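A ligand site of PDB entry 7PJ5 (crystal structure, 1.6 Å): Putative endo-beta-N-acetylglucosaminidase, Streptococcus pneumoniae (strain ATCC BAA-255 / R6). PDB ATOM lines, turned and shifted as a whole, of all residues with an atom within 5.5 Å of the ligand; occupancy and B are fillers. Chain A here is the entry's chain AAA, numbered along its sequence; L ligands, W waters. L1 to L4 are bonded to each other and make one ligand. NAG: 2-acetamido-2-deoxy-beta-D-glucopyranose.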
ATOM      1  N   THR A  11      15.602  19.171 -13.147  1.00  0.00           N
ATOM      2  CA  THR A  11      14.837  19.827 -12.088  1.00  0.00           C
ATOM      3  C   THR A  11      13.573  20.429 -12.698  1.00  0.00           C
ATOM      4  O   THR A  11      13.521  20.720 -13.928  1.00  0.00           O
ATOM      5  CB  THR A  11      15.633  20.911 -11.346  1.00  0.00           C
ATOM      6  OG1 THR A  11      15.860  22.007 -12.221  1.00  0.00           O
ATOM      7  CG2 THR A  11      16.954  20.428 -10.788  1.00  0.00           C
ATOM      8  N   TYR A  24      12.239  24.456  -6.307  1.00  0.00           N
ATOM      9  CA  TYR A  24      12.586  23.546  -7.414  1.00  0.00           C
ATOM     10  C   TYR A  24      12.820  22.171  -6.817  1.00  0.00           C
ATOM     11  O   TYR A  24      13.288  22.078  -5.665  1.00  0.00           O
ATOM     12  CB  TYR A  24      13.810  24.075  -8.156  1.00  0.00           C
ATOM     13  CG  TYR A  24      15.109  24.067  -7.405  1.00  0.00           C
ATOM     14  CD1 TYR A  24      15.344  24.853  -6.290  1.00  0.00           C
ATOM     15  CD2 TYR A  24      16.136  23.255  -7.832  1.00  0.00           C
ATOM     16  CE1 TYR A  24      16.551  24.791  -5.614  1.00  0.00           C
ATOM     17  CE2 TYR A  24      17.342  23.202  -7.176  1.00  0.00           C
ATOM     18  CZ  TYR A  24      17.569  23.958  -6.050  1.00  0.00           C
ATOM     19  OH  TYR A  24      18.763  23.909  -5.367  1.00  0.00           O
ATOM     20  N   SER A  26      13.977  17.825  -7.724  1.00  0.00           N
ATOM     21  CA  SER A  26      14.833  16.955  -8.535  1.00  0.00           C
ATOM     22  C   SER A  26      14.023  15.963  -9.411  1.00  0.00           C
ATOM     23  O   SER A  26      12.969  15.486  -9.029  1.00  0.00           O
ATOM     24  CB  SER A  26      15.770  16.221  -7.632  1.00  0.00           C
ATOM     25  OG  SER A  26      15.047  15.463  -6.683  1.00  0.00           O
ATOM     26  N   VAL A  84      13.075   7.076   0.678  1.00  0.00           N
ATOM     27  CA  VAL A  84      13.192   8.221  -0.265  1.00  0.00           C
ATOM     28  C   VAL A  84      13.415   7.707  -1.675  1.00  0.00           C
ATOM     29  O   VAL A  84      13.195   8.498  -2.615  1.00  0.00           O
ATOM     30  CB  VAL A  84      14.285   9.196   0.200  1.00  0.00           C
ATOM     31  CG1 VAL A  84      13.867   9.829   1.532  1.00  0.00           C
ATOM     32  CG2 VAL A  84      15.660   8.520   0.317  1.00  0.00           C
ATOM     33  N   ALA A  88      16.449   2.747  -0.802  1.00  0.00           N
ATOM     34  CA  ALA A  88      17.207   3.607   0.129  1.00  0.00           C
ATOM     35  C   ALA A  88      16.269   4.220   1.164  1.00  0.00           C
ATOM     36  O   ALA A  88      15.286   4.838   0.827  1.00  0.00           O
ATOM     37  CB  ALA A  88      17.952   4.685  -0.602  1.00  0.00           C
ATOM     38  N   SER A  89      16.611   4.000   2.418  1.00  0.00           N
ATOM     39  CA  SER A  89      15.853   4.521   3.565  1.00  0.00           C
ATOM     40  C   SER A  89      16.771   5.311   4.505  1.00  0.00           C
ATOM     41  O   SER A  89      17.980   5.045   4.579  1.00  0.00           O
ATOM     42  CB  SER A  89      15.148   3.435   4.304  1.00  0.00           C
ATOM     43  OG  SER A  89      16.039   2.461   4.855  1.00  0.00           O
ATOM     44  N   ILE A  90      16.162   6.273   5.198  1.00  0.00           N
ATOM     45  CA  ILE A  90      16.896   7.047   6.238  1.00  0.00           C
ATOM     46  C   ILE A  90      16.051   7.049   7.514  1.00  0.00           C
ATOM     47  O   ILE A  90      14.824   7.188   7.469  1.00  0.00           O
ATOM     48  CB  ILE A  90      17.238   8.456   5.771  1.00  0.00           C
ATOM     49  CG1 ILE A  90      15.950   9.213   5.447  1.00  0.00           C
ATOM     50  CG2 ILE A  90      18.214   8.464   4.585  1.00  0.00           C
ATOM     51  CD1 ILE A  90      16.163  10.697   5.189  1.00  0.00           C
ATOM     52  N   ALA A 178      28.987  15.318   5.879  1.00  0.00           N
ATOM     53  CA  ALA A 178      28.861  13.853   5.712  1.00  0.00           C
ATOM     54  C   ALA A 178      27.913  13.540   4.557  1.00  0.00           C
ATOM     55  O   ALA A 178      28.238  12.696   3.707  1.00  0.00           O
ATOM     56  CB  ALA A 178      28.306  13.249   6.977  1.00  0.00           C
ATOM     57  N   LEU A 179      26.742  14.178   4.526  1.00  0.00           N
ATOM     58  CA  LEU A 179      25.741  13.864   3.494  1.00  0.00           C
ATOM     59  C   LEU A 179      26.231  14.378   2.130  1.00  0.00           C
ATOM     60  O   LEU A 179      26.083  13.690   1.115  1.00  0.00           O
ATOM     61  CB  LEU A 179      24.387  14.503   3.869  1.00  0.00           C
ATOM     62  CG  LEU A 179      23.390  14.351   2.722  1.00  0.00           C
ATOM     63  CD1 LEU A 179      22.959  12.902   2.623  1.00  0.00           C
ATOM     64  CD2 LEU A 179      22.244  15.314   2.712  1.00  0.00           C
ATOM     65  N   GLU A 180      26.757  15.586   2.089  1.00  0.00           N
ATOM     66  CA  GLU A 180      27.014  16.241   0.785  1.00  0.00           C
ATOM     67  C   GLU A 180      28.200  15.612   0.078  1.00  0.00           C
ATOM     68  O   GLU A 180      28.217  15.599  -1.145  1.00  0.00           O
ATOM     69  CB  GLU A 180      27.323  17.707   1.040  1.00  0.00           C
ATOM     70  CG  GLU A 180      27.100  18.552  -0.168  1.00  0.00           C
ATOM     71  CD  GLU A 180      25.643  18.936  -0.471  1.00  0.00           C
ATOM     72  OE1 GLU A 180      24.886  19.338   0.474  1.00  0.00           O
ATOM     73  OE2 GLU A 180      25.332  18.967  -1.664  1.00  0.00           O
ATOM     74  N   SER A 181      29.179  15.148   0.824  1.00  0.00           N
ATOM     75  CA  SER A 181      30.498  14.722   0.251  1.00  0.00           C
ATOM     76  C   SER A 181      30.835  13.264   0.576  1.00  0.00           C
ATOM     77  O   SER A 181      31.999  12.905   0.484  1.00  0.00           O
ATOM     78  CB  SER A 181      31.590  15.657   0.675  1.00  0.00           C
ATOM     79  OG  SER A 181      31.880  15.560   2.057  1.00  0.00           O
ATOM     80  N   ASN A 182      29.880  12.489   1.040  1.00  0.00           N
ATOM     81  CA  ASN A 182      30.144  11.107   1.512  1.00  0.00           C
ATOM     82  C   ASN A 182      31.264  11.159   2.568  1.00  0.00           C
ATOM     83  O   ASN A 182      32.295  10.523   2.416  1.00  0.00           O
ATOM     84  CB  ASN A 182      30.470  10.185   0.356  1.00  0.00           C
ATOM     85  CG  ASN A 182      30.646   8.770   0.833  1.00  0.00           C
ATOM     86  OD1 ASN A 182      30.189   8.411   1.926  1.00  0.00           O
ATOM     87  ND2 ASN A 182      31.421   7.997   0.085  1.00  0.00           N
ATOM     88  N   TRP A 183      31.084  11.957   3.605  1.00  0.00           N
ATOM     89  CA  TRP A 183      32.077  12.052   4.710  1.00  0.00           C
ATOM     90  C   TRP A 183      33.434  12.468   4.144  1.00  0.00           C
ATOM     91  O   TRP A 183      34.462  11.909   4.542  1.00  0.00           O
ATOM     92  CB  TRP A 183      32.159  10.712   5.485  1.00  0.00           C
ATOM     93  CG  TRP A 183      30.905  10.335   6.203  1.00  0.00           C
ATOM     94  CD1 TRP A 183      29.827   9.634   5.721  1.00  0.00           C
ATOM     95  CD2 TRP A 183      30.626  10.610   7.576  1.00  0.00           C
ATOM     96  NE1 TRP A 183      28.889   9.482   6.710  1.00  0.00           N
ATOM     97  CE2 TRP A 183      29.341  10.090   7.853  1.00  0.00           C
ATOM     98  CE3 TRP A 183      31.309  11.312   8.569  1.00  0.00           C
ATOM     99  CZ2 TRP A 183      28.758  10.215   9.120  1.00  0.00           C
ATOM    100  CZ3 TRP A 183      30.744  11.401   9.822  1.00  0.00           C
ATOM    101  CH2 TRP A 183      29.484  10.874  10.075  1.00  0.00           C
ATOM    102  N   SER A 186      34.111  12.047  -1.471  1.00  0.00           N
ATOM    103  CA  SER A 186      33.701  12.252  -2.881  1.00  0.00           C
ATOM    104  C   SER A 186      34.902  12.810  -3.662  1.00  0.00           C
ATOM    105  O   SER A 186      35.920  13.273  -3.087  1.00  0.00           O
ATOM    106  CB  SER A 186      32.523  13.183  -2.949  1.00  0.00           C
ATOM    107  OG  SER A 186      32.925  14.510  -2.604  1.00  0.00           O
ATOM    108  N   PHE A 196      30.933  20.584   1.141  1.00  0.00           N
ATOM    109  CA  PHE A 196      29.559  21.113   1.316  1.00  0.00           C
ATOM    110  C   PHE A 196      28.919  21.390  -0.043  1.00  0.00           C
ATOM    111  O   PHE A 196      27.807  21.954  -0.080  1.00  0.00           O
ATOM    112  CB  PHE A 196      29.577  22.365   2.189  1.00  0.00           C
ATOM    113  CG  PHE A 196      30.053  22.145   3.583  1.00  0.00           C
ATOM    114  CD1 PHE A 196      31.404  22.091   3.904  1.00  0.00           C
ATOM    115  CD2 PHE A 196      29.125  21.907   4.579  1.00  0.00           C
ATOM    116  CE1 PHE A 196      31.808  21.905   5.214  1.00  0.00           C
ATOM    117  CE2 PHE A 196      29.542  21.718   5.892  1.00  0.00           C
ATOM    118  CZ  PHE A 196      30.878  21.717   6.200  1.00  0.00           C
ATOM    119  N   GLY A 197      29.584  20.996  -1.148  1.00  0.00           N
ATOM    120  CA  GLY A 197      28.939  21.116  -2.458  1.00  0.00           C
ATOM    121  C   GLY A 197      28.903  22.554  -2.989  1.00  0.00           C
ATOM    122  O   GLY A 197      28.082  22.866  -3.835  1.00  0.00           O
ATOM    123  N   ILE A 198      29.793  23.417  -2.539  1.00  0.00           N
ATOM    124  CA  ILE A 198      29.758  24.842  -2.937  1.00  0.00           C
ATOM    125  C   ILE A 198      30.363  24.987  -4.339  1.00  0.00           C
ATOM    126  O   ILE A 198      31.406  24.440  -4.603  1.00  0.00           O
ATOM    127  CB  ILE A 198      30.436  25.698  -1.869  1.00  0.00           C
ATOM    128  CG1 ILE A 198      29.738  25.520  -0.522  1.00  0.00           C
ATOM    129  CG2 ILE A 198      30.488  27.156  -2.302  1.00  0.00           C
ATOM    130  CD1 ILE A 198      30.470  26.174   0.590  1.00  0.00           C
ATOM    131  N   THR A 199      29.711  25.779  -5.174  1.00  0.00           N
ATOM    132  CA  THR A 199      30.154  25.998  -6.568  1.00  0.00           C
ATOM    133  C   THR A 199      30.618  27.428  -6.735  1.00  0.00           C
ATOM    134  O   THR A 199      30.228  28.283  -5.915  1.00  0.00           O
ATOM    135  CB  THR A 199      28.995  25.728  -7.532  1.00  0.00           C
ATOM    136  OG1 THR A 199      28.018  26.712  -7.151  1.00  0.00           O
ATOM    137  CG2 THR A 199      28.468  24.311  -7.449  1.00  0.00           C
ATOM    138  N   TRP A 225      30.782  30.744   3.871  1.00  0.00           N
ATOM    139  CA  TRP A 225      29.905  30.827   2.694  1.00  0.00           C
ATOM    140  C   TRP A 225      28.469  30.512   3.096  1.00  0.00           C
ATOM    141  O   TRP A 225      27.571  31.240   2.696  1.00  0.00           O
ATOM    142  CB  TRP A 225      30.403  29.866   1.626  1.00  0.00           C
ATOM    143  CG  TRP A 225      29.719  30.072   0.310  1.00  0.00           C
ATOM    144  CD1 TRP A 225      30.141  30.840  -0.747  1.00  0.00           C
ATOM    145  CD2 TRP A 225      28.432  29.540  -0.090  1.00  0.00           C
ATOM    146  NE1 TRP A 225      29.235  30.787  -1.764  1.00  0.00           N
ATOM    147  CE2 TRP A 225      28.189  29.973  -1.402  1.00  0.00           C
ATOM    148  CE3 TRP A 225      27.529  28.658   0.523  1.00  0.00           C
ATOM    149  CZ2 TRP A 225      27.045  29.601  -2.098  1.00  0.00           C
ATOM    150  CZ3 TRP A 225      26.398  28.283  -0.171  1.00  0.00           C
ATOM    151  CH2 TRP A 225      26.148  28.773  -1.460  1.00  0.00           C
ATOM    152  N   TYR A 230      23.225  31.804   3.412  1.00  0.00           N
ATOM    153  CA  TYR A 230      22.009  31.159   3.958  1.00  0.00           C
ATOM    154  C   TYR A 230      21.646  31.761   5.311  1.00  0.00           C
ATOM    155  O   TYR A 230      20.536  32.323   5.448  1.00  0.00           O
ATOM    156  CB  TYR A 230      22.180  29.635   4.009  1.00  0.00           C
ATOM    157  CG  TYR A 230      21.981  29.031   2.636  1.00  0.00           C
ATOM    158  CD1 TYR A 230      22.976  29.092   1.669  1.00  0.00           C
ATOM    159  CD2 TYR A 230      20.742  28.572   2.252  1.00  0.00           C
ATOM    160  CE1 TYR A 230      22.744  28.648   0.365  1.00  0.00           C
ATOM    161  CE2 TYR A 230      20.483  28.154   0.963  1.00  0.00           C
ATOM    162  CZ  TYR A 230      21.492  28.155   0.016  1.00  0.00           C
ATOM    163  OH  TYR A 230      21.212  27.730  -1.246  1.00  0.00           O
ATOM    164  N   GLU A 248      16.397  26.440  -1.195  1.00  0.00           N
ATOM    165  CA  GLU A 248      17.374  26.879  -2.236  1.00  0.00           C
ATOM    166  C   GLU A 248      18.556  25.933  -2.355  1.00  0.00           C
ATOM    167  O   GLU A 248      19.150  25.857  -3.440  1.00  0.00           O
ATOM    168  CB  GLU A 248      17.889  28.290  -1.968  1.00  0.00           C
ATOM    169  CG  GLU A 248      16.800  29.321  -2.049  1.00  0.00           C
ATOM    170  CD  GLU A 248      16.075  29.608  -0.753  1.00  0.00           C
ATOM    171  OE1 GLU A 248      16.517  29.130   0.318  1.00  0.00           O
ATOM    172  OE2 GLU A 248      15.084  30.376  -0.819  1.00  0.00           O
ATOM    173  N   TYR A 249      18.976  25.224  -1.300  1.00  0.00           N
ATOM    174  CA  TYR A 249      20.335  24.592  -1.319  1.00  0.00           C
ATOM    175  C   TYR A 249      20.411  23.440  -2.305  1.00  0.00           C
ATOM    176  O   TYR A 249      21.508  23.189  -2.913  1.00  0.00           O
ATOM    177  CB  TYR A 249      20.742  24.120   0.092  1.00  0.00           C
ATOM    178  CG  TYR A 249      22.228  24.030   0.286  1.00  0.00           C
ATOM    179  CD1 TYR A 249      22.967  22.936  -0.121  1.00  0.00           C
ATOM    180  CD2 TYR A 249      22.907  25.051   0.922  1.00  0.00           C
ATOM    181  CE1 TYR A 249      24.338  22.875   0.055  1.00  0.00           C
ATOM    182  CE2 TYR A 249      24.257  25.002   1.146  1.00  0.00           C
ATOM    183  CZ  TYR A 249      24.994  23.935   0.661  1.00  0.00           C
ATOM    184  OH  TYR A 249      26.347  23.933   0.918  1.00  0.00           O
ATOM    185  N   ALA A 250      19.326  22.673  -2.405  1.00  0.00           N
ATOM    186  CA  ALA A 250      19.343  21.397  -3.144  1.00  0.00           C
ATOM    187  C   ALA A 250      17.989  21.144  -3.778  1.00  0.00           C
ATOM    188  O   ALA A 250      16.958  21.518  -3.185  1.00  0.00           O
ATOM    189  CB  ALA A 250      19.681  20.284  -2.208  1.00  0.00           C
ATOM    190  N   SER A 251      17.999  20.504  -4.945  1.00  0.00           N
ATOM    191  CA  SER A 251      16.740  20.094  -5.621  1.00  0.00           C
ATOM    192  C   SER A 251      16.076  18.933  -4.867  1.00  0.00           C
ATOM    193  O   SER A 251      14.864  18.845  -4.923  1.00  0.00           O
ATOM    194  CB  SER A 251      16.953  19.723  -7.056  1.00  0.00           C
ATOM    195  OG  SER A 251      17.918  18.668  -7.193  1.00  0.00           O
ATOM    196  N   ASP A 252      16.861  18.093  -4.199  1.00  0.00           N
ATOM    197  CA  ASP A 252      16.371  16.925  -3.440  1.00  0.00           C
ATOM    198  C   ASP A 252      15.400  17.463  -2.389  1.00  0.00           C
ATOM    199  O   ASP A 252      15.817  18.194  -1.502  1.00  0.00           O
ATOM    200  CB  ASP A 252      17.561  16.222  -2.785  1.00  0.00           C
ATOM    201  CG  ASP A 252      17.267  14.982  -1.975  1.00  0.00           C
ATOM    202  OD1 ASP A 252      16.086  14.617  -1.839  1.00  0.00           O
ATOM    203  OD2 ASP A 252      18.253  14.388  -1.511  1.00  0.00           O
ATOM    204  N   TRP A 255      16.756  16.562   1.151  1.00  0.00           N
ATOM    205  CA  TRP A 255      18.147  16.921   1.555  1.00  0.00           C
ATOM    206  C   TRP A 255      18.149  17.251   3.049  1.00  0.00           C
ATOM    207  O   TRP A 255      19.048  16.784   3.790  1.00  0.00           O
ATOM    208  CB  TRP A 255      18.583  18.092   0.662  1.00  0.00           C
ATOM    209  CG  TRP A 255      19.865  18.769   1.013  1.00  0.00           C
ATOM    210  CD1 TRP A 255      21.120  18.469   0.595  1.00  0.00           C
ATOM    211  CD2 TRP A 255      19.967  19.904   1.864  1.00  0.00           C
ATOM    212  NE1 TRP A 255      22.012  19.374   1.114  1.00  0.00           N
ATOM    213  CE2 TRP A 255      21.326  20.287   1.889  1.00  0.00           C
ATOM    214  CE3 TRP A 255      19.022  20.640   2.611  1.00  0.00           C
ATOM    215  CZ2 TRP A 255      21.777  21.364   2.662  1.00  0.00           C
ATOM    216  CZ3 TRP A 255      19.470  21.690   3.372  1.00  0.00           C
ATOM    217  CH2 TRP A 255      20.831  22.043   3.396  1.00  0.00           C
ATOM    218  N   LYS A 258      17.703  14.199   5.183  1.00  0.00           N
ATOM    219  CA  LYS A 258      18.929  13.392   5.173  1.00  0.00           C
ATOM    220  C   LYS A 258      19.971  13.954   6.143  1.00  0.00           C
ATOM    221  O   LYS A 258      20.607  13.180   6.888  1.00  0.00           O
ATOM    222  CB  LYS A 258      19.465  13.320   3.751  1.00  0.00           C
ATOM    223  CG  LYS A 258      18.643  12.460   2.810  1.00  0.00           C
ATOM    224  CD  LYS A 258      19.137  12.554   1.401  1.00  0.00           C
ATOM    225  CE  LYS A 258      18.329  11.701   0.473  1.00  0.00           C
ATOM    226  NZ  LYS A 258      18.761  11.852  -0.933  1.00  0.00           N
HETATM  227  C1  NAG L   1      23.649   8.931  -0.160  1.00  0.00           C
HETATM  228  C2  NAG L   1      22.537   9.983  -0.100  1.00  0.00           C
HETATM  229  C3  NAG L   1      22.816  10.999  -1.176  1.00  0.00           C
HETATM  230  C4  NAG L   1      24.228  11.558  -1.090  1.00  0.00           C
HETATM  231  C5  NAG L   1      25.242  10.425  -0.994  1.00  0.00           C
HETATM  232  C6  NAG L   1      26.667  10.912  -0.785  1.00  0.00           C
HETATM  233  C7  NAG L   1      20.541   8.875   0.790  1.00  0.00           C
HETATM  234  C8  NAG L   1      19.383   7.995   0.421  1.00  0.00           C
HETATM  235  N2  NAG L   1      21.243   9.347  -0.271  1.00  0.00           N
HETATM  236  O1  NAG L   1      23.593   8.128   0.978  1.00  0.00           O
HETATM  237  O3  NAG L   1      21.773  12.001  -1.035  1.00  0.00           O
HETATM  238  O4  NAG L   1      24.558  12.328  -2.269  1.00  0.00           O
HETATM  239  O5  NAG L   1      24.897   9.536   0.064  1.00  0.00           O
HETATM  240  O6  NAG L   1      26.893  11.280   0.587  1.00  0.00           O
HETATM  241  O7  NAG L   1      20.855   9.187   1.954  1.00  0.00           O
HETATM  242  C1  NAG L   2      24.437  13.756  -2.192  1.00  0.00           C
HETATM  243  C2  NAG L   2      25.283  14.313  -3.302  1.00  0.00           C
HETATM  244  C3  NAG L   2      25.039  15.804  -3.429  1.00  0.00           C
HETATM  245  C4  NAG L   2      23.556  16.114  -3.596  1.00  0.00           C
HETATM  246  C5  NAG L   2      22.833  15.466  -2.425  1.00  0.00           C
HETATM  247  C6  NAG L   2      21.313  15.683  -2.466  1.00  0.00           C
HETATM  248  C7  NAG L   2      27.511  13.118  -3.655  1.00  0.00           C
HETATM  249  C8  NAG L   2      26.875  12.315  -4.656  1.00  0.00           C
HETATM  250  N2  NAG L   2      26.686  14.013  -3.083  1.00  0.00           N
HETATM  251  O3  NAG L   2      25.737  16.281  -4.617  1.00  0.00           O
HETATM  252  O4  NAG L   2      23.273  17.529  -3.494  1.00  0.00           O
HETATM  253  O5  NAG L   2      23.080  14.061  -2.446  1.00  0.00           O
HETATM  254  O6  NAG L   2      20.789  15.153  -1.246  1.00  0.00           O
HETATM  255  O7  NAG L   2      28.770  12.987  -3.315  1.00  0.00           O
HETATM  256  C1  NAG L   3      23.425  18.339  -4.661  1.00  0.00           C
HETATM  257  C2  NAG L   3      22.053  18.808  -5.123  1.00  0.00           C
HETATM  258  C3  NAG L   3      22.060  20.039  -6.011  1.00  0.00           C
HETATM  259  C4  NAG L   3      22.930  21.104  -5.403  1.00  0.00           C
HETATM  260  C5  NAG L   3      24.305  20.473  -5.169  1.00  0.00           C
HETATM  261  C6  NAG L   3      25.281  21.468  -4.572  1.00  0.00           C
HETATM  262  C7  NAG L   3      20.220  17.225  -5.440  1.00  0.00           C
HETATM  263  C8  NAG L   3      19.680  16.101  -6.295  1.00  0.00           C
HETATM  264  N2  NAG L   3      21.414  17.698  -5.829  1.00  0.00           N
HETATM  265  O3  NAG L   3      20.718  20.469  -6.181  1.00  0.00           O
HETATM  266  O4  NAG L   3      23.160  22.153  -6.350  1.00  0.00           O
HETATM  267  O5  NAG L   3      24.212  19.412  -4.222  1.00  0.00           O
HETATM  268  O6  NAG L   3      26.610  20.888  -4.683  1.00  0.00           O
HETATM  269  O7  NAG L   3      19.651  17.761  -4.493  1.00  0.00           O
HETATM  270  C1  NAG L   4      22.179  23.182  -6.420  1.00  0.00           C
HETATM  271  C2  NAG L   4      22.836  24.500  -5.997  1.00  0.00           C
HETATM  272  C3  NAG L   4      21.834  25.636  -6.187  1.00  0.00           C
HETATM  273  C4  NAG L   4      21.360  25.608  -7.661  1.00  0.00           C
HETATM  274  C5  NAG L   4      20.793  24.257  -8.051  1.00  0.00           C
HETATM  275  C6  NAG L   4      20.512  24.166  -9.524  1.00  0.00           C
HETATM  276  C7  NAG L   4      24.494  25.000  -4.264  1.00  0.00           C
HETATM  277  C8  NAG L   4      24.758  24.990  -2.809  1.00  0.00           C
HETATM  278  N2  NAG L   4      23.320  24.530  -4.648  1.00  0.00           N
HETATM  279  O3  NAG L   4      22.481  26.879  -5.870  1.00  0.00           O
HETATM  280  O4  NAG L   4      20.338  26.601  -7.825  1.00  0.00           O
HETATM  281  O5  NAG L   4      21.800  23.245  -7.796  1.00  0.00           O
HETATM  282  O6  NAG L   4      19.869  22.930  -9.818  1.00  0.00           O
HETATM  283  O7  NAG L   4      25.335  25.398  -5.068  1.00  0.00           O
HETATM  284  O   HOH W   1      19.075  27.669  -5.520  1.00  0.00           O
HETATM  285  O   HOH W   2      27.317  18.349  -3.812  1.00  0.00           O
HETATM  286  O   HOH W   3      27.405  26.817  -4.323  1.00  0.00           O
HETATM  287  O   HOH W   4      23.289  21.616  -9.701  1.00  0.00           O
HETATM  288  O   HOH W   5      20.040  20.388  -8.915  1.00  0.00           O
HETATM  289  O   HOH W   6      22.728  16.803  -8.292  1.00  0.00           O
HETATM  290  O   HOH W   7      20.759  27.888  -9.870  1.00  0.00           O
HETATM  291  O   HOH W   8      22.947  28.018  -3.236  1.00  0.00           O
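An oxygen (O6) of NAG L1 is in hydrogen-bond range of the backbone carbonyl oxygen of Leu 179 (2.6 Å).
The backbone carbonyl oxygen of Gly 197 is in hydrogen-bond range of an oxygen (O6) of NAG L3, at 2.6 Å.
The backbone NH (N) of Asp 252 lies within hydrogen-bond range of an oxygen (O7) of NAG L3, 2.8 Å away.
OD2 of Asp 252 sits at hydrogen-bond distance from O6 of NAG L2 (2.7 Å).
O of Glu 180 sits at hydrogen-bond distance from N2 of NAG L2, 2.9 Å away.
O of Tyr 249 is in hydrogen-bond range of N2 of NAG L4 (2.8 Å).
The backbone NH (N) of Ser 251 sits at hydrogen-bond distance from an oxygen (O3) of NAG L3 (3.0 Å).
O7 of NAG L3 lies close to OG of Ser 251, at 3.3 Å.
NZ of Lys 258 sits at hydrogen-bond distance from O3 of NAG L1.
N of Asn 182 sits at hydrogen-bond distance from O6 of NAG L1 (3.3 Å).
NZ of Lys 258 is in salt-bridge range of OD2 of Asp 252, at 2.7 Å.
The indole nitrogen (NE1) of Trp 255 lies within hydrogen-bond range of the side-chain carboxylate (OE1) of Glu 180, 2.9 Å away.
The backbone NH (N) of Tyr 249 lies close to the side-chain hydroxyl (OH) of Tyr 230 (3.4 Å).
The backbone carbonyl oxygen (O) of Phe 196 is in hydrogen-bond range of the side-chain hydroxyl (OH) of Tyr 249 (2.7 Å).
N of Ser 26 lies within hydrogen-bond range of O of Ser 251.
OH of Tyr 24 is in hydrogen-bond range of N of Ala 250 (3.3 Å).
The side-chain hydroxyl (OH) of Tyr 24 is in hydrogen-bond range of the backbone carbonyl oxygen (O) of Glu 248 (2.8 Å).
The backbone carbonyl oxygen of Ala 178 is in hydrogen-bond range of the backbone NH of Trp 183, 2.9 Å away.
Residues that only touch the ligand: Thr 11, Tyr 24, Val 84, Ala 88, Ile 90, Ala 178, Ser 186, Thr 199, Glu 248, Ala 250 and Trp 255.
Hydrophobic or aromatic side chains within 4 Å of the ligand: Tyr 24, Val 84, Ala 88, Ile 90, Leu 179, Tyr 249, Ala 250 and Trp 255.
Of the 27 residues printed, 19 come within 4 Å of the ligand.
Along chain A the residues within 4 Å of the ligand span positions 11 to 258.
The nearest printed residue that does not touch the ligand is Ser 26 (4.1 Å).
Water W3 bridges an oxygen (O7) of NAG L4 (2.6 Å) and the backbone NH (N) of Thr 199 (2.7 Å).
Water W5 lies within hydrogen-bond range of an oxygen (O6) of NAG L4 (2.7 Å) and the side-chain hydroxyl (OG) of Ser 251 (3.2 Å).
Water W2 bridges an oxygen (O3) of NAG L2 (2.7 Å) and the side-chain carboxylate (OE2) of Glu 180 (3.0 Å).
Water W1 lies within hydrogen-bond range of the backbone carbonyl oxygen of Glu 248 and an oxygen (O4) of NAG L4.
Water W8 bridges the side-chain hydroxyl of Tyr 230 and an oxygen (O3) of NAG L4.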
